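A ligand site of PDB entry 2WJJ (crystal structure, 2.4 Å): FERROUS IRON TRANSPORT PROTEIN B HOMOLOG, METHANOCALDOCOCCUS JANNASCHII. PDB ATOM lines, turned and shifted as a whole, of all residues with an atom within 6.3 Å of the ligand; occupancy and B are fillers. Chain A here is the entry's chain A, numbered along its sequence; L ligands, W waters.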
ATOM      1  N   ASN A  12     -15.392 -13.793 -15.063  1.00  0.00           N
ATOM      2  CA  ASN A  12     -15.917 -12.554 -14.497  1.00  0.00           C
ATOM      3  C   ASN A  12     -14.783 -11.674 -14.013  1.00  0.00           C
ATOM      4  O   ASN A  12     -13.674 -12.139 -13.754  1.00  0.00           O
ATOM      5  CB  ASN A  12     -16.846 -12.807 -13.309  1.00  0.00           C
ATOM      6  CG  ASN A  12     -18.068 -13.646 -13.651  1.00  0.00           C
ATOM      7  OD1 ASN A  12     -18.240 -14.080 -14.787  1.00  0.00           O
ATOM      8  ND2 ASN A  12     -18.911 -13.879 -12.655  1.00  0.00           N
ATOM      9  N   PRO A  13     -15.060 -10.369 -13.853  1.00  0.00           N
ATOM     10  CA  PRO A  13     -14.090  -9.483 -13.224  1.00  0.00           C
ATOM     11  C   PRO A  13     -13.791  -9.947 -11.802  1.00  0.00           C
ATOM     12  O   PRO A  13     -14.681 -10.501 -11.159  1.00  0.00           O
ATOM     13  CB  PRO A  13     -14.826  -8.137 -13.194  1.00  0.00           C
ATOM     14  CG  PRO A  13     -15.821  -8.230 -14.316  1.00  0.00           C
ATOM     15  CD  PRO A  13     -16.272  -9.655 -14.309  1.00  0.00           C
ATOM     16  N   ASN A  14     -12.561  -9.748 -11.326  1.00  0.00           N
ATOM     17  CA  ASN A  14     -12.225  -9.981  -9.915  1.00  0.00           C
ATOM     18  C   ASN A  14     -12.188 -11.443  -9.482  1.00  0.00           C
ATOM     19  O   ASN A  14     -12.375 -11.726  -8.316  1.00  0.00           O
ATOM     20  CB  ASN A  14     -13.216  -9.256  -9.020  1.00  0.00           C
ATOM     21  CG  ASN A  14     -12.633  -8.884  -7.680  1.00  0.00           C
ATOM     22  OD1 ASN A  14     -11.573  -8.257  -7.615  1.00  0.00           O
ATOM     23  ND2 ASN A  14     -13.325  -9.264  -6.599  1.00  0.00           N
ATOM     24  N   VAL A  15     -11.952 -12.359 -10.404  1.00  0.00           N
ATOM     25  CA  VAL A  15     -11.936 -13.767 -10.051  1.00  0.00           C
ATOM     26  C   VAL A  15     -10.523 -14.293  -9.832  1.00  0.00           C
ATOM     27  O   VAL A  15     -10.364 -15.437  -9.460  1.00  0.00           O
ATOM     28  CB  VAL A  15     -12.624 -14.669 -11.107  1.00  0.00           C
ATOM     29  CG1 VAL A  15     -14.109 -14.381 -11.176  1.00  0.00           C
ATOM     30  CG2 VAL A  15     -11.969 -14.499 -12.485  1.00  0.00           C
ATOM     31  N   GLY A  16      -9.519 -13.445 -10.079  1.00  0.00           N
ATOM     32  CA  GLY A  16      -8.133 -13.868  -9.992  1.00  0.00           C
ATOM     33  C   GLY A  16      -7.489 -14.183 -11.344  1.00  0.00           C
ATOM     34  O   GLY A  16      -6.485 -14.907 -11.423  1.00  0.00           O
ATOM     35  N   LYS A  17      -8.050 -13.643 -12.407  1.00  0.00           N
ATOM     36  CA  LYS A  17      -7.530 -13.914 -13.741  1.00  0.00           C
ATOM     37  C   LYS A  17      -6.138 -13.312 -13.919  1.00  0.00           C
ATOM     38  O   LYS A  17      -5.219 -13.915 -14.491  1.00  0.00           O
ATOM     39  CB  LYS A  17      -8.504 -13.365 -14.775  1.00  0.00           C
ATOM     40  CG  LYS A  17      -8.302 -13.898 -16.164  1.00  0.00           C
ATOM     41  CD  LYS A  17      -9.629 -14.009 -16.924  1.00  0.00           C
ATOM     42  CE  LYS A  17     -10.390 -12.686 -16.973  1.00  0.00           C
ATOM     43  NZ  LYS A  17      -9.571 -11.565 -17.508  1.00  0.00           N
ATOM     44  N   SER A  18      -5.968 -12.099 -13.418  1.00  0.00           N
ATOM     45  CA  SER A  18      -4.693 -11.445 -13.508  1.00  0.00           C
ATOM     46  C   SER A  18      -3.653 -12.200 -12.638  1.00  0.00           C
ATOM     47  O   SER A  18      -2.492 -12.388 -13.029  1.00  0.00           O
ATOM     48  CB  SER A  18      -4.862  -9.999 -13.083  1.00  0.00           C
ATOM     49  OG  SER A  18      -3.716  -9.256 -13.429  1.00  0.00           O
ATOM     50  N   THR A  19      -4.085 -12.658 -11.465  1.00  0.00           N
ATOM     51  CA  THR A  19      -3.206 -13.398 -10.563  1.00  0.00           C
ATOM     52  C   THR A  19      -2.764 -14.724 -11.182  1.00  0.00           C
ATOM     53  O   THR A  19      -1.597 -15.117 -11.075  1.00  0.00           O
ATOM     54  CB  THR A  19      -3.927 -13.641  -9.230  1.00  0.00           C
ATOM     55  OG1 THR A  19      -4.195 -12.382  -8.614  1.00  0.00           O
ATOM     56  CG2 THR A  19      -3.076 -14.514  -8.296  1.00  0.00           C
ATOM     57  N   ILE A  20      -3.703 -15.411 -11.836  1.00  0.00           N
ATOM     58  CA  ILE A  20      -3.381 -16.672 -12.486  1.00  0.00           C
ATOM     59  C   ILE A  20      -2.510 -16.449 -13.715  1.00  0.00           C
ATOM     60  O   ILE A  20      -1.596 -17.223 -13.963  1.00  0.00           O
ATOM     61  CB  ILE A  20      -4.630 -17.470 -12.851  1.00  0.00           C
ATOM     62  CG1 ILE A  20      -5.208 -18.101 -11.583  1.00  0.00           C
ATOM     63  CG2 ILE A  20      -4.284 -18.563 -13.857  1.00  0.00           C
ATOM     64  CD1 ILE A  20      -6.670 -18.454 -11.659  1.00  0.00           C
ATOM     65  N   LYS A  42      -3.380  -8.337 -22.430  1.00  0.00           N
ATOM     66  CA  LYS A  42      -2.195  -9.017 -21.901  1.00  0.00           C
ATOM     67  C   LYS A  42      -1.948 -10.332 -22.620  1.00  0.00           C
ATOM     68  O   LYS A  42      -2.839 -11.168 -22.724  1.00  0.00           O
ATOM     69  CB  LYS A  42      -2.333  -9.253 -20.401  1.00  0.00           C
ATOM     70  CG  LYS A  42      -1.524  -8.311 -19.541  1.00  0.00           C
ATOM     71  CD  LYS A  42      -2.246  -7.960 -18.246  1.00  0.00           C
ATOM     72  CE  LYS A  42      -2.456  -9.158 -17.370  1.00  0.00           C
ATOM     73  NZ  LYS A  42      -3.635  -8.937 -16.496  1.00  0.00           N
ATOM     74  N   ASP A  57      -4.913 -13.140 -22.218  1.00  0.00           N
ATOM     75  CA  ASP A  57      -5.907 -12.745 -21.227  1.00  0.00           C
ATOM     76  C   ASP A  57      -7.055 -12.001 -21.909  1.00  0.00           C
ATOM     77  O   ASP A  57      -6.874 -10.903 -22.441  1.00  0.00           O
ATOM     78  CB  ASP A  57      -5.265 -11.863 -20.157  1.00  0.00           C
ATOM     79  CG  ASP A  57      -6.136 -11.710 -18.937  1.00  0.00           C
ATOM     80  OD1 ASP A  57      -7.079 -12.501 -18.796  1.00  0.00           O
ATOM     81  OD2 ASP A  57      -5.863 -10.816 -18.107  1.00  0.00           O
ATOM     82  N   ILE A  89     -11.855 -19.188 -15.801  1.00  0.00           N
ATOM     83  CA  ILE A  89     -11.553 -18.971 -14.399  1.00  0.00           C
ATOM     84  C   ILE A  89     -12.792 -18.537 -13.650  1.00  0.00           C
ATOM     85  O   ILE A  89     -13.412 -17.525 -13.962  1.00  0.00           O
ATOM     86  CB  ILE A  89     -10.414 -17.966 -14.235  1.00  0.00           C
ATOM     87  CG1 ILE A  89      -9.171 -18.489 -14.952  1.00  0.00           C
ATOM     88  CG2 ILE A  89     -10.159 -17.687 -12.754  1.00  0.00           C
ATOM     89  CD1 ILE A  89      -8.063 -17.495 -15.001  1.00  0.00           C
ATOM     90  N   ASN A 117     -11.038 -21.053  -8.836  1.00  0.00           N
ATOM     91  CA  ASN A 117     -10.153 -20.278  -7.996  1.00  0.00           C
ATOM     92  C   ASN A 117     -10.786 -19.853  -6.662  1.00  0.00           C
ATOM     93  O   ASN A 117     -11.996 -19.956  -6.460  1.00  0.00           O
ATOM     94  CB  ASN A 117      -9.634 -19.052  -8.745  1.00  0.00           C
ATOM     95  CG  ASN A 117      -8.395 -18.457  -8.100  1.00  0.00           C
ATOM     96  OD1 ASN A 117      -7.617 -19.168  -7.470  1.00  0.00           O
ATOM     97  ND2 ASN A 117      -8.219 -17.144  -8.254  1.00  0.00           N
ATOM     98  N   LYS A 118      -9.931 -19.386  -5.746  1.00  0.00           N
ATOM     99  CA  LYS A 118     -10.361 -18.841  -4.472  1.00  0.00           C
ATOM    100  C   LYS A 118     -10.919 -19.892  -3.484  1.00  0.00           C
ATOM    101  O   LYS A 118     -11.772 -19.604  -2.635  1.00  0.00           O
ATOM    102  CB  LYS A 118     -11.363 -17.701  -4.698  1.00  0.00           C
ATOM    103  CG  LYS A 118     -10.796 -16.529  -5.505  1.00  0.00           C
ATOM    104  CD  LYS A 118     -11.439 -15.208  -5.107  1.00  0.00           C
ATOM    105  CE  LYS A 118     -11.072 -14.076  -6.070  1.00  0.00           C
ATOM    106  NZ  LYS A 118     -11.604 -12.744  -5.603  1.00  0.00           N
ATOM    107  N   MET A 119     -10.432 -21.124  -3.608  1.00  0.00           N
ATOM    108  CA  MET A 119     -10.841 -22.220  -2.717  1.00  0.00           C
ATOM    109  C   MET A 119     -10.591 -21.890  -1.245  1.00  0.00           C
ATOM    110  O   MET A 119     -11.379 -22.262  -0.366  1.00  0.00           O
ATOM    111  CB  MET A 119     -10.135 -23.524  -3.088  1.00  0.00           C
ATOM    112  CG  MET A 119     -10.533 -24.084  -4.452  1.00  0.00           C
ATOM    113  SD  MET A 119     -12.403 -24.644  -4.488  1.00  0.00           S
ATOM    114  CE  MET A 119     -12.219 -26.424  -3.574  1.00  0.00           C
ATOM    115  N   ASP A 120      -9.513 -21.170  -0.967  1.00  0.00           N
ATOM    116  CA  ASP A 120      -9.220 -20.733   0.386  1.00  0.00           C
ATOM    117  C   ASP A 120     -10.311 -19.815   0.933  1.00  0.00           C
ATOM    118  O   ASP A 120     -10.780 -19.993   2.043  1.00  0.00           O
ATOM    119  CB  ASP A 120      -7.863 -20.027   0.445  1.00  0.00           C
ATOM    120  CG  ASP A 120      -7.864 -18.698  -0.316  1.00  0.00           C
ATOM    121  OD1 ASP A 120      -7.613 -17.653   0.320  1.00  0.00           O
ATOM    122  OD2 ASP A 120      -8.105 -18.714  -1.550  1.00  0.00           O
ATOM    123  N   LEU A 121     -10.698 -18.823   0.132  1.00  0.00           N
ATOM    124  CA  LEU A 121     -11.691 -17.854   0.550  1.00  0.00           C
ATOM    125  C   LEU A 121     -13.010 -18.539   0.848  1.00  0.00           C
ATOM    126  O   LEU A 121     -13.664 -18.258   1.855  1.00  0.00           O
ATOM    127  CB  LEU A 121     -11.886 -16.803  -0.540  1.00  0.00           C
ATOM    128  CG  LEU A 121     -12.111 -15.348  -0.134  1.00  0.00           C
ATOM    129  CD1 LEU A 121     -13.166 -14.771  -1.039  1.00  0.00           C
ATOM    130  CD2 LEU A 121     -12.534 -15.160   1.313  1.00  0.00           C
ATOM    131  N   LEU A 145      -8.203 -24.323  -7.113  1.00  0.00           N
ATOM    132  CA  LEU A 145      -6.966 -23.671  -6.708  1.00  0.00           C
ATOM    133  C   LEU A 145      -7.158 -22.436  -5.838  1.00  0.00           C
ATOM    134  O   LEU A 145      -8.299 -22.005  -5.581  1.00  0.00           O
ATOM    135  CB  LEU A 145      -6.073 -23.348  -7.910  1.00  0.00           C
ATOM    136  CG  LEU A 145      -6.410 -22.284  -8.957  1.00  0.00           C
ATOM    137  CD1 LEU A 145      -5.161 -21.970  -9.777  1.00  0.00           C
ATOM    138  CD2 LEU A 145      -7.505 -22.738  -9.875  1.00  0.00           C
ATOM    139  N   SER A 146      -6.030 -21.927  -5.351  1.00  0.00           N
ATOM    140  CA  SER A 146      -5.956 -20.642  -4.666  1.00  0.00           C
ATOM    141  C   SER A 146      -4.701 -19.922  -5.164  1.00  0.00           C
ATOM    142  O   SER A 146      -3.621 -20.037  -4.585  1.00  0.00           O
ATOM    143  CB  SER A 146      -5.907 -20.833  -3.142  1.00  0.00           C
ATOM    144  OG  SER A 146      -7.029 -21.591  -2.695  1.00  0.00           O
ATOM    145  N   ALA A 147      -4.862 -19.181  -6.265  1.00  0.00           N
ATOM    146  CA  ALA A 147      -3.745 -18.617  -6.996  1.00  0.00           C
ATOM    147  C   ALA A 147      -2.973 -17.614  -6.141  1.00  0.00           C
ATOM    148  O   ALA A 147      -1.752 -17.527  -6.246  1.00  0.00           O
ATOM    149  CB  ALA A 147      -4.231 -17.947  -8.293  1.00  0.00           C
ATOM    150  N   ALA A 148      -3.687 -16.873  -5.301  1.00  0.00           N
ATOM    151  CA  ALA A 148      -3.055 -15.850  -4.486  1.00  0.00           C
ATOM    152  C   ALA A 148      -2.146 -16.479  -3.443  1.00  0.00           C
ATOM    153  O   ALA A 148      -1.157 -15.875  -3.012  1.00  0.00           O
ATOM    154  CB  ALA A 148      -4.114 -14.948  -3.818  1.00  0.00           C
ATOM    155  N   LYS A 149      -2.484 -17.701  -3.022  1.00  0.00           N
ATOM    156  CA  LYS A 149      -1.654 -18.444  -2.080  1.00  0.00           C
ATOM    157  C   LYS A 149      -0.782 -19.437  -2.799  1.00  0.00           C
ATOM    158  O   LYS A 149      -0.300 -20.383  -2.212  1.00  0.00           O
ATOM    159  CB  LYS A 149      -2.517 -19.168  -1.054  1.00  0.00           C
ATOM    160  CG  LYS A 149      -3.228 -18.230  -0.101  1.00  0.00           C
ATOM    161  CD  LYS A 149      -4.158 -18.965   0.831  1.00  0.00           C
ATOM    162  CE  LYS A 149      -3.394 -19.733   1.903  1.00  0.00           C
ATOM    163  NZ  LYS A 149      -4.316 -20.257   2.952  1.00  0.00           N
HETATM  164  P1  LIG L   1      -9.127 -10.325 -11.984  1.00  0.00           P
HETATM  165  O1  LIG L   1      -8.028 -10.240 -13.013  1.00  0.00           O
HETATM  166  O2  LIG L   1     -10.004 -11.495 -12.341  1.00  0.00           O
HETATM  167  O3  LIG L   1      -9.879  -9.021 -11.979  1.00  0.00           O
HETATM  168  O4  LIG L   1      -8.671 -10.612 -10.477  1.00  0.00           O
HETATM  169  P2  LIG L   1      -7.238 -10.324  -9.805  1.00  0.00           P
HETATM  170  O5  LIG L   1      -6.751  -8.909  -9.877  1.00  0.00           O
HETATM  171  O6  LIG L   1      -6.231 -11.294 -10.367  1.00  0.00           O
HETATM  172  O7  LIG L   1      -7.689 -10.672  -8.303  1.00  0.00           O
HETATM  173  C1  LIG L   1      -8.599  -9.794  -7.648  1.00  0.00           C
HETATM  174  C2  LIG L   1      -8.435  -9.919  -6.140  1.00  0.00           C
HETATM  175  O8  LIG L   1      -8.657 -11.274  -5.739  1.00  0.00           O
HETATM  176  C3  LIG L   1      -7.018  -9.586  -5.732  1.00  0.00           C
HETATM  177  O9  LIG L   1      -7.081  -8.895  -4.486  1.00  0.00           O
HETATM  178  C4  LIG L   1      -6.355 -10.941  -5.545  1.00  0.00           C
HETATM  179  O10 LIG L   1      -5.337 -10.933  -4.550  1.00  0.00           O
HETATM  180  C5  LIG L   1      -7.524 -11.746  -5.042  1.00  0.00           C
HETATM  181  N1  LIG L   1      -7.271 -13.156  -5.345  1.00  0.00           N
HETATM  182  C6  LIG L   1      -6.804 -13.694  -6.473  1.00  0.00           C
HETATM  183  N2  LIG L   1      -6.709 -15.033  -6.336  1.00  0.00           N
HETATM  184  C7  LIG L   1      -7.099 -15.363  -5.094  1.00  0.00           C
HETATM  185  C8  LIG L   1      -7.231 -16.590  -4.289  1.00  0.00           C
HETATM  186  O11 LIG L   1      -6.950 -17.706  -4.774  1.00  0.00           O
HETATM  187  N3  LIG L   1      -7.690 -16.454  -3.044  1.00  0.00           N
HETATM  188  C9  LIG L   1      -8.016 -15.254  -2.499  1.00  0.00           C
HETATM  189  N4  LIG L   1      -8.465 -15.183  -1.229  1.00  0.00           N
HETATM  190  N5  LIG L   1      -7.900 -14.092  -3.170  1.00  0.00           N
HETATM  191  C10 LIG L   1      -7.464 -14.101  -4.450  1.00  0.00           C
HETATM  192  O   HOH W   1      -9.802  -7.162  -9.914  1.00  0.00           O
HETATM  193  O   HOH W   2      -9.894 -11.948  -2.652  1.00  0.00           O
HETATM  194  O   HOH W   3     -11.198 -11.212 -14.734  1.00  0.00           O
HETATM  195  O   HOH W   4      -5.538 -10.935  -1.757  1.00  0.00           O
HETATM  196  O   HOH W   5      -7.711  -9.917 -15.557  1.00  0.00           O
HETATM  197  O   HOH W   6      -5.063  -7.214  -4.029  1.00  0.00           O
HETATM  198  O   HOH W   7      -8.922 -12.095   0.086  1.00  0.00           O
HETATM  199  O   HOH W   8      -9.386  -8.976  -3.152  1.00  0.00           O
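Water W5 lies within hydrogen-bond range of an oxygen (O1) of the ligand (2.6 Å), the side-chain amino group (NZ) of Lys 17 (3.2 Å) and the side-chain carboxylate (OD2) of Asp 57 (3.3 Å).
Water W3 lies within hydrogen-bond range of O2 of the ligand, O of Asn 12 and NZ of Lys 17.
Water W1 lies within hydrogen-bond range of an oxygen (O3) of the ligand (2.8 Å) and the side-chain amide oxygen of Asn 14 (3.1 Å).
Merely in contact with the ligand: Ser 146, Leu 121 and Asn 12.
Within 4 Å of the ligand: Asn 12, Asn 14, Val 15, Gly 16, Lys 17, Ser 18, Thr 19, Asn 117, Lys 118, Asp 120, Leu 121, Ser 146, Ala 147 and Ala 148.
The nearest printed residue that does not touch the ligand is Pro 13 (4.02 Å).
The side-chain hydroxyl of Ser 146 sits at hydrogen-bond distance from the backbone NH of Asp 120.
The side-chain hydroxyl (OG) of Ser 18 lies within hydrogen-bond range of the side-chain amino group (NZ) of Lys 42, at 3.1 Å.
The backbone carbonyl oxygen of Asn 14 sits at hydrogen-bond distance from the side-chain amino group of Lys 118, 3.0 Å away.
ND2 of Asn 117 sits at hydrogen-bond distance from O of Val 15 (3.0 Å).
The side-chain amino group of Lys 17 is in salt-bridge range of the side-chain carboxylate of Asp 57, at 3.0 Å.
OD1 of Asn 117 is in hydrogen-bond range of N of Ala 147, 3.0 Å away.
The side-chain amide oxygen (OD1) of Asn 117 sits close to the backbone carbonyl oxygen (O) of Leu 145 (3.5 Å).
The backbone NH (N) of Lys 118 sits at hydrogen-bond distance from the backbone carbonyl oxygen (O) of Leu 145, at 3.1 Å.
The side-chain carboxylate (OD2) of Asp 120 is in hydrogen-bond range of a nitrogen (N3) of the ligand (2.7 Å).
O6 of the ligand sits at hydrogen-bond distance from N of Thr 19.
OG1 of Thr 19 is in hydrogen-bond range of O6 of the ligand.
N of Ser 18 lies within hydrogen-bond range of O1 of the ligand, 2.8 Å away.
N of Asn 14 lies within hydrogen-bond range of O3 of the ligand, at 2.9 Å.
O2 of the ligand lies within hydrogen-bond range of N of Val 15 (2.9 Å).
O2 of the ligand lies within hydrogen-bond range of N of Lys 17 (2.9 Å).
O11 of the ligand lies within hydrogen-bond range of N of Ala 147 (3.0 Å).
N of Gly 16 lies within hydrogen-bond range of O4 of the ligand, at 3.0 Å.
The side-chain amide oxygen (OD1) of Asn 117 lies close to an oxygen (O11) of the ligand, 3.1 Å away.
The backbone NH (N) of Ala 148 sits at hydrogen-bond distance from an oxygen (O11) of the ligand, at 3.4 Å.
NZ of Lys 118 lies within hydrogen-bond range of O8 of the ligand.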
